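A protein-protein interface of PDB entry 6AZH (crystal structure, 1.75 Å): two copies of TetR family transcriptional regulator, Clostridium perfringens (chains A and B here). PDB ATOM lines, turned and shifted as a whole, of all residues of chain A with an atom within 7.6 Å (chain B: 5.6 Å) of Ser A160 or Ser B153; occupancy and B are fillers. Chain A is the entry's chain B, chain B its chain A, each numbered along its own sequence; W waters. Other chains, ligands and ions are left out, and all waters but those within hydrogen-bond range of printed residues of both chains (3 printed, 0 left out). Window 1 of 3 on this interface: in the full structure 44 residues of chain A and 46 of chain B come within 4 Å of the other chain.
Among the printed residues, merely in contact across the chains: Ser A160 with Gly B156, Tyr A164 with Ser B148, Tyr A164 with Leu B149, Tyr A164 with His B152, Ser A160 with His B152, Ser A160 with Ser B153, Ile A181 with Ser B153, Asn A184 with Leu B150 and Leu A163 with Phe B155.
Water W1 bridges the side-chain hydroxyl of Ser A160 and the backbone carbonyl oxygen of Ser B153.
Water W2 bridges O of Ile B185 (2.8 Å) and O of Asn A184 (2.8 Å).
Water W3 lies within hydrogen-bond range of the side-chain amide nitrogen (ND2) of Asn A184 (2.9 Å) and the side-chain hydroxyl (OG) of Ser B153 (3.1 Å).
Of chain B, only His B152 (3.5 Å), Ser B153 (3.7 Å) and Gly B156 (3.1 Å) come within 4 Å of Ser A160.
Printed residues of chain B within 4 Å of Leu A163: Phe B155.
Of the printed residues of chain B, Ile A181 touches Ser B153.
Printed residues of chain B within 4 Å of Asn A184: Leu B150 (3.8 Å).
Of the printed residues of chain A, Ser B148 touches Tyr A164.
Printed residues of chain A within 4 Å of His B152: Ser A160 (3.5 Å) and Tyr A164 (3.5 Å).
Of the printed residues of chain A, Ser B153 touches Ser A160 and Ile A181.
The nearest residue of chain A that does not touch Ser B153 is Asn A184 (5.3 Å).
O of Ser B148 lies within hydrogen-bond range of ND1 of His B152 (2.9 Å).
OG of Ser B153 lies within hydrogen-bond range of O of Leu B149, at 3.4 Å.
The backbone carbonyl oxygen of Gly A156 lies within hydrogen-bond range of the side-chain hydroxyl of Ser A160, at 3.1 Å.
O of Leu A163 sits at hydrogen-bond distance from OG of Ser A167 (3.0 Å).
Of the 21 printed residues of chain A, 5 touch a printed residue of chain B.
Of the 11 printed residues of chain B, 7 touch a printed residue of chain A.
Hydrophobic or aromatic side chains of chain B within 4 Å of the printed part of chain A: Leu B149, Leu B150, His B152 and Phe B155.
Among the printed residues, no Asp or Glu carboxylate lies within 4 Å of a Lys or Arg side-chain nitrogen of the other chain.
5 positions are printed for both chains.
Of the 9 pairs that touch across the chains among the printed residues, none has its exchanged pair printed and touching as well.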
ATOM      1  N   PHE A  91     -24.476 -22.532   6.335  1.00  0.00           N
ATOM      2  CA  PHE A  91     -23.632 -23.461   7.076  1.00  0.00           C
ATOM      3  C   PHE A  91     -23.819 -24.885   6.571  1.00  0.00           C
ATOM      4  O   PHE A  91     -22.853 -25.652   6.487  1.00  0.00           O
ATOM      5  CB  PHE A  91     -23.923 -23.346   8.579  1.00  0.00           C
ATOM      6  CG  PHE A  91     -23.258 -22.160   9.228  1.00  0.00           C
ATOM      7  CD1 PHE A  91     -21.876 -22.041   9.225  1.00  0.00           C
ATOM      8  CD2 PHE A  91     -24.013 -21.164   9.829  1.00  0.00           C
ATOM      9  CE1 PHE A  91     -21.267 -20.955   9.819  1.00  0.00           C
ATOM     10  CE2 PHE A  91     -23.399 -20.072  10.421  1.00  0.00           C
ATOM     11  CZ  PHE A  91     -22.031 -19.968  10.408  1.00  0.00           C
ATOM     12  N   LEU A  94     -21.856 -24.978   3.325  1.00  0.00           N
ATOM     13  CA  LEU A  94     -20.441 -25.012   3.679  1.00  0.00           C
ATOM     14  C   LEU A  94     -20.008 -26.426   4.032  1.00  0.00           C
ATOM     15  O   LEU A  94     -18.950 -26.892   3.592  1.00  0.00           O
ATOM     16  CB  LEU A  94     -20.170 -24.070   4.855  1.00  0.00           C
ATOM     17  CG  LEU A  94     -18.734 -23.930   5.373  1.00  0.00           C
ATOM     18  CD1 LEU A  94     -17.702 -23.628   4.291  1.00  0.00           C
ATOM     19  CD2 LEU A  94     -18.690 -22.868   6.456  1.00  0.00           C
ATOM     20  N   PHE A 101     -15.193 -24.649  -0.885  1.00  0.00           N
ATOM     21  CA  PHE A 101     -15.119 -23.378  -0.172  1.00  0.00           C
ATOM     22  C   PHE A 101     -13.675 -22.977   0.107  1.00  0.00           C
ATOM     23  O   PHE A 101     -13.277 -21.835  -0.142  1.00  0.00           O
ATOM     24  CB  PHE A 101     -15.909 -23.447   1.128  1.00  0.00           C
ATOM     25  CG  PHE A 101     -16.090 -22.104   1.773  1.00  0.00           C
ATOM     26  CD1 PHE A 101     -17.130 -21.269   1.385  1.00  0.00           C
ATOM     27  CD2 PHE A 101     -15.199 -21.655   2.737  1.00  0.00           C
ATOM     28  CE1 PHE A 101     -17.287 -20.016   1.964  1.00  0.00           C
ATOM     29  CE2 PHE A 101     -15.355 -20.402   3.322  1.00  0.00           C
ATOM     30  CZ  PHE A 101     -16.397 -19.588   2.928  1.00  0.00           C
ATOM     31  N   MET A 105     -11.493 -19.685  -1.067  1.00  0.00           N
ATOM     32  CA  MET A 105     -10.772 -18.814  -0.130  1.00  0.00           C
ATOM     33  C   MET A 105      -9.300 -18.634  -0.493  1.00  0.00           C
ATOM     34  O   MET A 105      -8.762 -17.538  -0.366  1.00  0.00           O
ATOM     35  CB  MET A 105     -10.845 -19.353   1.306  1.00  0.00           C
ATOM     36  CG  MET A 105     -12.220 -19.358   1.964  1.00  0.00           C
ATOM     37  SD  MET A 105     -13.000 -17.529   2.010  1.00  0.00           S
ATOM     38  CE  MET A 105     -14.205 -17.652   0.570  1.00  0.00           C
ATOM     39  N   SER A 153     -20.196  -9.204   6.242  1.00  0.00           N
ATOM     40  CA  SER A 153     -20.031  -9.840   7.550  1.00  0.00           C
ATOM     41  C   SER A 153     -20.841 -11.128   7.659  1.00  0.00           C
ATOM     42  O   SER A 153     -20.396 -12.092   8.292  1.00  0.00           O
ATOM     43  CB  SER A 153     -20.438  -8.878   8.676  1.00  0.00           C
ATOM     44  OG  SER A 153     -19.558  -7.776   8.758  1.00  0.00           O
ATOM     45  N   PHE A 155     -21.687 -13.183   5.120  1.00  0.00           N
ATOM     46  CA  PHE A 155     -20.880 -14.172   4.412  1.00  0.00           C
ATOM     47  C   PHE A 155     -19.651 -14.543   5.236  1.00  0.00           C
ATOM     48  O   PHE A 155     -19.260 -15.717   5.292  1.00  0.00           O
ATOM     49  CB  PHE A 155     -20.486 -13.627   3.033  1.00  0.00           C
ATOM     50  CG  PHE A 155     -19.687 -14.592   2.205  1.00  0.00           C
ATOM     51  CD1 PHE A 155     -20.291 -15.691   1.617  1.00  0.00           C
ATOM     52  CD2 PHE A 155     -18.331 -14.392   2.007  1.00  0.00           C
ATOM     53  CE1 PHE A 155     -19.535 -16.576   0.844  1.00  0.00           C
ATOM     54  CE2 PHE A 155     -17.583 -15.265   1.241  1.00  0.00           C
ATOM     55  CZ  PHE A 155     -18.186 -16.352   0.663  1.00  0.00           C
ATOM     56  N   GLY A 156     -19.081 -13.564   5.945  1.00  0.00           N
ATOM     57  CA  GLY A 156     -17.909 -13.805   6.775  1.00  0.00           C
ATOM     58  C   GLY A 156     -18.109 -14.841   7.867  1.00  0.00           C
ATOM     59  O   GLY A 156     -17.141 -15.429   8.342  1.00  0.00           O
ATOM     60  N   SER A 157     -19.356 -15.059   8.309  1.00  0.00           N
ATOM     61  CA  SER A 157     -19.591 -16.103   9.302  1.00  0.00           C
ATOM     62  C   SER A 157     -19.120 -17.467   8.801  1.00  0.00           C
ATOM     63  O   SER A 157     -18.644 -18.287   9.596  1.00  0.00           O
ATOM     64  CB  SER A 157     -21.081 -16.135   9.697  1.00  0.00           C
ATOM     65  OG  SER A 157     -21.892 -16.612   8.631  1.00  0.00           O
ATOM     66  N   LEU A 158     -19.218 -17.720   7.488  1.00  0.00           N
ATOM     67  CA  LEU A 158     -18.722 -18.970   6.932  1.00  0.00           C
ATOM     68  C   LEU A 158     -17.207 -18.969   6.873  1.00  0.00           C
ATOM     69  O   LEU A 158     -16.572 -19.995   7.122  1.00  0.00           O
ATOM     70  CB  LEU A 158     -19.269 -19.190   5.522  1.00  0.00           C
ATOM     71  CG  LEU A 158     -20.758 -19.059   5.301  1.00  0.00           C
ATOM     72  CD1 LEU A 158     -21.009 -19.161   3.801  1.00  0.00           C
ATOM     73  CD2 LEU A 158     -21.471 -20.174   6.052  1.00  0.00           C
ATOM     74  N   ILE A 159     -16.621 -17.827   6.510  1.00  0.00           N
ATOM     75  CA  ILE A 159     -15.164 -17.722   6.453  1.00  0.00           C
ATOM     76  C   ILE A 159     -14.561 -18.029   7.819  1.00  0.00           C
ATOM     77  O   ILE A 159     -13.624 -18.831   7.940  1.00  0.00           O
ATOM     78  CB  ILE A 159     -14.742 -16.329   5.959  1.00  0.00           C
ATOM     79  CG1 ILE A 159     -15.340 -16.025   4.578  1.00  0.00           C
ATOM     80  CG2 ILE A 159     -13.197 -16.232   5.964  1.00  0.00           C
ATOM     81  CD1 ILE A 159     -15.106 -14.612   4.146  1.00  0.00           C
ATOM     82  N   SER A 160     -15.099 -17.399   8.871  1.00  0.00           N
ATOM     83  CA  SER A 160     -14.595 -17.612  10.224  1.00  0.00           C
ATOM     84  C   SER A 160     -14.751 -19.065  10.654  1.00  0.00           C
ATOM     85  O   SER A 160     -13.838 -19.654  11.249  1.00  0.00           O
ATOM     86  CB  SER A 160     -15.345 -16.710  11.217  1.00  0.00           C
ATOM     87  OG  SER A 160     -15.279 -15.355  10.829  1.00  0.00           O
ATOM     88  N   THR A 161     -15.928 -19.639  10.424  1.00  0.00           N
ATOM     89  CA  THR A 161     -16.150 -21.025  10.830  1.00  0.00           C
ATOM     90  C   THR A 161     -15.220 -21.973  10.082  1.00  0.00           C
ATOM     91  O   THR A 161     -14.630 -22.878  10.684  1.00  0.00           O
ATOM     92  CB  THR A 161     -17.617 -21.398  10.611  1.00  0.00           C
ATOM     93  OG1 THR A 161     -18.427 -20.582  11.463  1.00  0.00           O
ATOM     94  CG2 THR A 161     -17.866 -22.868  10.938  1.00  0.00           C
ATOM     95  N   SER A 162     -15.063 -21.766   8.774  1.00  0.00           N
ATOM     96  CA  SER A 162     -14.151 -22.592   7.989  1.00  0.00           C
ATOM     97  C   SER A 162     -12.717 -22.493   8.524  1.00  0.00           C
ATOM     98  O   SER A 162     -12.016 -23.509   8.655  1.00  0.00           O
ATOM     99  CB  SER A 162     -14.250 -22.171   6.520  1.00  0.00           C
ATOM    100  OG  SER A 162     -13.342 -22.878   5.716  1.00  0.00           O
ATOM    101  N   LEU A 163     -12.274 -21.278   8.874  1.00  0.00           N
ATOM    102  CA  LEU A 163     -10.933 -21.113   9.433  1.00  0.00           C
ATOM    103  C   LEU A 163     -10.815 -21.797  10.790  1.00  0.00           C
ATOM    104  O   LEU A 163      -9.803 -22.442  11.088  1.00  0.00           O
ATOM    105  CB  LEU A 163     -10.593 -19.632   9.569  1.00  0.00           C
ATOM    106  CG  LEU A 163      -9.247 -19.338  10.243  1.00  0.00           C
ATOM    107  CD1 LEU A 163      -8.091 -19.982   9.491  1.00  0.00           C
ATOM    108  CD2 LEU A 163      -9.024 -17.829  10.391  1.00  0.00           C
ATOM    109  N   TYR A 164     -11.845 -21.655  11.619  1.00  0.00           N
ATOM    110  CA  TYR A 164     -11.882 -22.291  12.929  1.00  0.00           C
ATOM    111  C   TYR A 164     -11.734 -23.804  12.802  1.00  0.00           C
ATOM    112  O   TYR A 164     -10.946 -24.433  13.517  1.00  0.00           O
ATOM    113  CB  TYR A 164     -13.209 -21.907  13.596  1.00  0.00           C
ATOM    114  CG  TYR A 164     -13.513 -22.462  14.979  1.00  0.00           C
ATOM    115  CD1 TYR A 164     -12.514 -22.738  15.894  1.00  0.00           C
ATOM    116  CD2 TYR A 164     -14.832 -22.668  15.368  1.00  0.00           C
ATOM    117  CE1 TYR A 164     -12.827 -23.223  17.167  1.00  0.00           C
ATOM    118  CE2 TYR A 164     -15.150 -23.144  16.626  1.00  0.00           C
ATOM    119  CZ  TYR A 164     -14.147 -23.425  17.518  1.00  0.00           C
ATOM    120  OH  TYR A 164     -14.483 -23.908  18.764  1.00  0.00           O
ATOM    121  N   GLU A 165     -12.477 -24.403  11.872  1.00  0.00           N
ATOM    122  CA  GLU A 165     -12.403 -25.845  11.684  1.00  0.00           C
ATOM    123  C   GLU A 165     -11.017 -26.264  11.221  1.00  0.00           C
ATOM    124  O   GLU A 165     -10.482 -27.283  11.674  1.00  0.00           O
ATOM    125  CB  GLU A 165     -13.465 -26.281  10.679  1.00  0.00           C
ATOM    126  CG  GLU A 165     -14.851 -26.285  11.281  1.00  0.00           C
ATOM    127  CD  GLU A 165     -15.912 -26.645  10.273  1.00  0.00           C
ATOM    128  OE1 GLU A 165     -15.607 -26.607   9.059  1.00  0.00           O
ATOM    129  OE2 GLU A 165     -17.044 -26.953  10.705  1.00  0.00           O
ATOM    130  N   LEU A 166     -10.413 -25.483  10.320  1.00  0.00           N
ATOM    131  CA  LEU A 166      -9.070 -25.816   9.846  1.00  0.00           C
ATOM    132  C   LEU A 166      -8.041 -25.704  10.963  1.00  0.00           C
ATOM    133  O   LEU A 166      -7.120 -26.522  11.062  1.00  0.00           O
ATOM    134  CB  LEU A 166      -8.672 -24.891   8.706  1.00  0.00           C
ATOM    135  CG  LEU A 166      -8.973 -25.340   7.291  1.00  0.00           C
ATOM    136  CD1 LEU A 166      -8.600 -24.198   6.351  1.00  0.00           C
ATOM    137  CD2 LEU A 166      -8.220 -26.630   6.954  1.00  0.00           C
ATOM    138  N   SER A 167      -8.169 -24.678  11.787  1.00  0.00           N
ATOM    139  CA  SER A 167      -7.161 -24.390  12.790  1.00  0.00           C
ATOM    140  C   SER A 167      -7.201 -25.400  13.934  1.00  0.00           C
ATOM    141  O   SER A 167      -6.162 -25.698  14.531  1.00  0.00           O
ATOM    142  CB  SER A 167      -7.361 -22.961  13.303  1.00  0.00           C
ATOM    143  OG  SER A 167      -7.125 -22.015  12.254  1.00  0.00           O
ATOM    144  N   ILE A 181     -24.141 -18.894  16.081  1.00  0.00           N
ATOM    145  CA  ILE A 181     -23.885 -17.770  15.183  1.00  0.00           C
ATOM    146  C   ILE A 181     -25.140 -16.922  15.023  1.00  0.00           C
ATOM    147  O   ILE A 181     -25.078 -15.688  15.061  1.00  0.00           O
ATOM    148  CB  ILE A 181     -23.357 -18.282  13.830  1.00  0.00           C
ATOM    149  CG1 ILE A 181     -21.998 -18.985  14.003  1.00  0.00           C
ATOM    150  CG2 ILE A 181     -23.286 -17.137  12.816  1.00  0.00           C
ATOM    151  CD1 ILE A 181     -20.868 -18.092  14.524  1.00  0.00           C
ATOM    152  N   ASN A 184     -25.530 -14.689  17.986  1.00  0.00           N
ATOM    153  CA  ASN A 184     -24.475 -13.672  17.968  1.00  0.00           C
ATOM    154  C   ASN A 184     -24.808 -12.567  16.975  1.00  0.00           C
ATOM    155  O   ASN A 184     -24.666 -11.377  17.276  1.00  0.00           O
ATOM    156  CB  ASN A 184     -23.123 -14.293  17.599  1.00  0.00           C
ATOM    157  CG  ASN A 184     -22.536 -15.157  18.695  1.00  0.00           C
ATOM    158  OD1 ASN A 184     -23.046 -15.210  19.805  1.00  0.00           O
ATOM    159  ND2 ASN A 184     -21.432 -15.835  18.378  1.00  0.00           N
ATOM    160  N   ILE A 185     -25.253 -12.949  15.774  1.00  0.00           N
ATOM    161  CA  ILE A 185     -25.498 -11.961  14.726  1.00  0.00           C
ATOM    162  C   ILE A 185     -26.728 -11.122  15.046  1.00  0.00           C
ATOM    163  O   ILE A 185     -26.702  -9.885  14.950  1.00  0.00           O
ATOM    164  CB  ILE A 185     -25.636 -12.657  13.361  1.00  0.00           C
ATOM    165  CG1 ILE A 185     -24.278 -13.217  12.928  1.00  0.00           C
ATOM    166  CG2 ILE A 185     -26.178 -11.694  12.327  1.00  0.00           C
ATOM    167  CD1 ILE A 185     -24.338 -14.014  11.641  1.00  0.00           C
ATOM    168  N   SER B 148     -14.275 -19.928  21.817  1.00  0.00           N
ATOM    169  CA  SER B 148     -13.411 -20.125  20.657  1.00  0.00           C
ATOM    170  C   SER B 148     -14.143 -19.794  19.361  1.00  0.00           C
ATOM    171  O   SER B 148     -13.577 -19.150  18.468  1.00  0.00           O
ATOM    172  CB  SER B 148     -12.891 -21.554  20.627  1.00  0.00           C
ATOM    173  OG  SER B 148     -11.917 -21.747  21.637  1.00  0.00           O
ATOM    174  N   LEU B 149     -15.388 -20.245  19.234  1.00  0.00           N
ATOM    175  CA  LEU B 149     -16.182 -19.897  18.063  1.00  0.00           C
ATOM    176  C   LEU B 149     -16.314 -18.386  17.934  1.00  0.00           C
ATOM    177  O   LEU B 149     -16.120 -17.830  16.849  1.00  0.00           O
ATOM    178  CB  LEU B 149     -17.561 -20.562  18.149  1.00  0.00           C
ATOM    179  CG  LEU B 149     -18.490 -20.377  16.954  1.00  0.00           C
ATOM    180  CD1 LEU B 149     -17.814 -20.910  15.698  1.00  0.00           C
ATOM    181  CD2 LEU B 149     -19.827 -21.084  17.158  1.00  0.00           C
ATOM    182  N   LEU B 150     -16.641 -17.704  19.039  1.00  0.00           N
ATOM    183  CA  LEU B 150     -16.780 -16.251  18.994  1.00  0.00           C
ATOM    184  C   LEU B 150     -15.459 -15.577  18.638  1.00  0.00           C
ATOM    185  O   LEU B 150     -15.416 -14.694  17.773  1.00  0.00           O
ATOM    186  CB  LEU B 150     -17.304 -15.730  20.333  1.00  0.00           C
ATOM    187  CG  LEU B 150     -17.485 -14.214  20.405  1.00  0.00           C
ATOM    188  CD1 LEU B 150     -18.374 -13.716  19.262  1.00  0.00           C
ATOM    189  CD2 LEU B 150     -18.091 -13.828  21.755  1.00  0.00           C
ATOM    190  N   ALA B 151     -14.365 -15.987  19.289  1.00  0.00           N
ATOM    191  CA  ALA B 151     -13.079 -15.352  19.016  1.00  0.00           C
ATOM    192  C   ALA B 151     -12.698 -15.488  17.549  1.00  0.00           C
ATOM    193  O   ALA B 151     -12.142 -14.557  16.957  1.00  0.00           O
ATOM    194  CB  ALA B 151     -11.984 -15.944  19.896  1.00  0.00           C
ATOM    195  N   HIS B 152     -12.999 -16.636  16.937  1.00  0.00           N
ATOM    196  CA  HIS B 152     -12.700 -16.764  15.512  1.00  0.00           C
ATOM    197  C   HIS B 152     -13.597 -15.868  14.673  1.00  0.00           C
ATOM    198  O   HIS B 152     -13.163 -15.362  13.636  1.00  0.00           O
ATOM    199  CB  HIS B 152     -12.837 -18.216  15.062  1.00  0.00           C
ATOM    200  CG  HIS B 152     -11.630 -19.040  15.367  1.00  0.00           C
ATOM    201  ND1 HIS B 152     -11.335 -19.472  16.640  1.00  0.00           N
ATOM    202  CD2 HIS B 152     -10.625 -19.481  14.575  1.00  0.00           C
ATOM    203  CE1 HIS B 152     -10.208 -20.165  16.616  1.00  0.00           C
ATOM    204  NE2 HIS B 152      -9.758 -20.187  15.375  1.00  0.00           N
ATOM    205  N   SER B 153     -14.841 -15.649  15.112  1.00  0.00           N
ATOM    206  CA  SER B 153     -15.722 -14.709  14.434  1.00  0.00           C
ATOM    207  C   SER B 153     -15.194 -13.288  14.537  1.00  0.00           C
ATOM    208  O   SER B 153     -15.338 -12.502  13.594  1.00  0.00           O
ATOM    209  CB  SER B 153     -17.140 -14.784  15.022  1.00  0.00           C
ATOM    210  OG  SER B 153     -17.783 -15.961  14.575  1.00  0.00           O
ATOM    211  N   LEU B 154     -14.609 -12.929  15.685  1.00  0.00           N
ATOM    212  CA  LEU B 154     -14.072 -11.581  15.842  1.00  0.00           C
ATOM    213  C   LEU B 154     -12.843 -11.379  14.974  1.00  0.00           C
ATOM    214  O   LEU B 154     -12.679 -10.318  14.361  1.00  0.00           O
ATOM    215  CB  LEU B 154     -13.732 -11.295  17.304  1.00  0.00           C
ATOM    216  CG  LEU B 154     -14.883 -11.403  18.294  1.00  0.00           C
ATOM    217  CD1 LEU B 154     -14.447 -10.786  19.608  1.00  0.00           C
ATOM    218  CD2 LEU B 154     -16.108 -10.721  17.725  1.00  0.00           C
ATOM    219  N   PHE B 155     -11.971 -12.392  14.894  1.00  0.00           N
ATOM    220  CA  PHE B 155     -10.874 -12.320  13.940  1.00  0.00           C
ATOM    221  C   PHE B 155     -11.402 -12.310  12.507  1.00  0.00           C
ATOM    222  O   PHE B 155     -10.920 -11.546  11.661  1.00  0.00           O
ATOM    223  CB  PHE B 155      -9.909 -13.488  14.136  1.00  0.00           C
ATOM    224  CG  PHE B 155      -8.745 -13.449  13.191  1.00  0.00           C
ATOM    225  CD1 PHE B 155      -7.677 -12.598  13.434  1.00  0.00           C
ATOM    226  CD2 PHE B 155      -8.739 -14.230  12.046  1.00  0.00           C
ATOM    227  CE1 PHE B 155      -6.609 -12.536  12.549  1.00  0.00           C
ATOM    228  CE2 PHE B 155      -7.683 -14.173  11.161  1.00  0.00           C
ATOM    229  CZ  PHE B 155      -6.616 -13.332  11.417  1.00  0.00           C
ATOM    230  N   GLY B 156     -12.413 -13.138  12.226  1.00  0.00           N
ATOM    231  CA  GLY B 156     -12.985 -13.241  10.898  1.00  0.00           C
ATOM    232  C   GLY B 156     -13.614 -11.965  10.378  1.00  0.00           C
ATOM    233  O   GLY B 156     -13.717 -11.799   9.159  1.00  0.00           O
ATOM    234  N   SER B 157     -14.017 -11.049  11.265  1.00  0.00           N
ATOM    235  CA  SER B 157     -14.442  -9.724  10.808  1.00  0.00           C
ATOM    236  C   SER B 157     -13.351  -9.031   9.990  1.00  0.00           C
ATOM    237  O   SER B 157     -13.662  -8.243   9.090  1.00  0.00           O
ATOM    238  CB  SER B 157     -14.862  -8.844  11.987  1.00  0.00           C
ATOM    239  OG  SER B 157     -13.751  -8.361  12.734  1.00  0.00           O
ATOM    240  N   ILE B 185     -21.417  -6.154  16.146  1.00  0.00           N
ATOM    241  CA  ILE B 185     -20.949  -7.275  16.958  1.00  0.00           C
ATOM    242  C   ILE B 185     -21.519  -7.203  18.372  1.00  0.00           C
ATOM    243  O   ILE B 185     -21.982  -8.209  18.923  1.00  0.00           O
ATOM    244  CB  ILE B 185     -19.409  -7.310  16.990  1.00  0.00           C
ATOM    245  CG1 ILE B 185     -18.839  -7.713  15.636  1.00  0.00           C
ATOM    246  CG2 ILE B 185     -18.940  -8.281  18.064  1.00  0.00           C
ATOM    247  CD1 ILE B 185     -17.322  -7.811  15.630  1.00  0.00           C
HETATM  248  O   HOH W   1     -16.834 -13.446  11.286  1.00  0.00           O
HETATM  249  O   HOH W   2     -22.031 -10.592  17.547  1.00  0.00           O
HETATM  250  O   HOH W   3     -20.264 -14.723  15.920  1.00  0.00           O
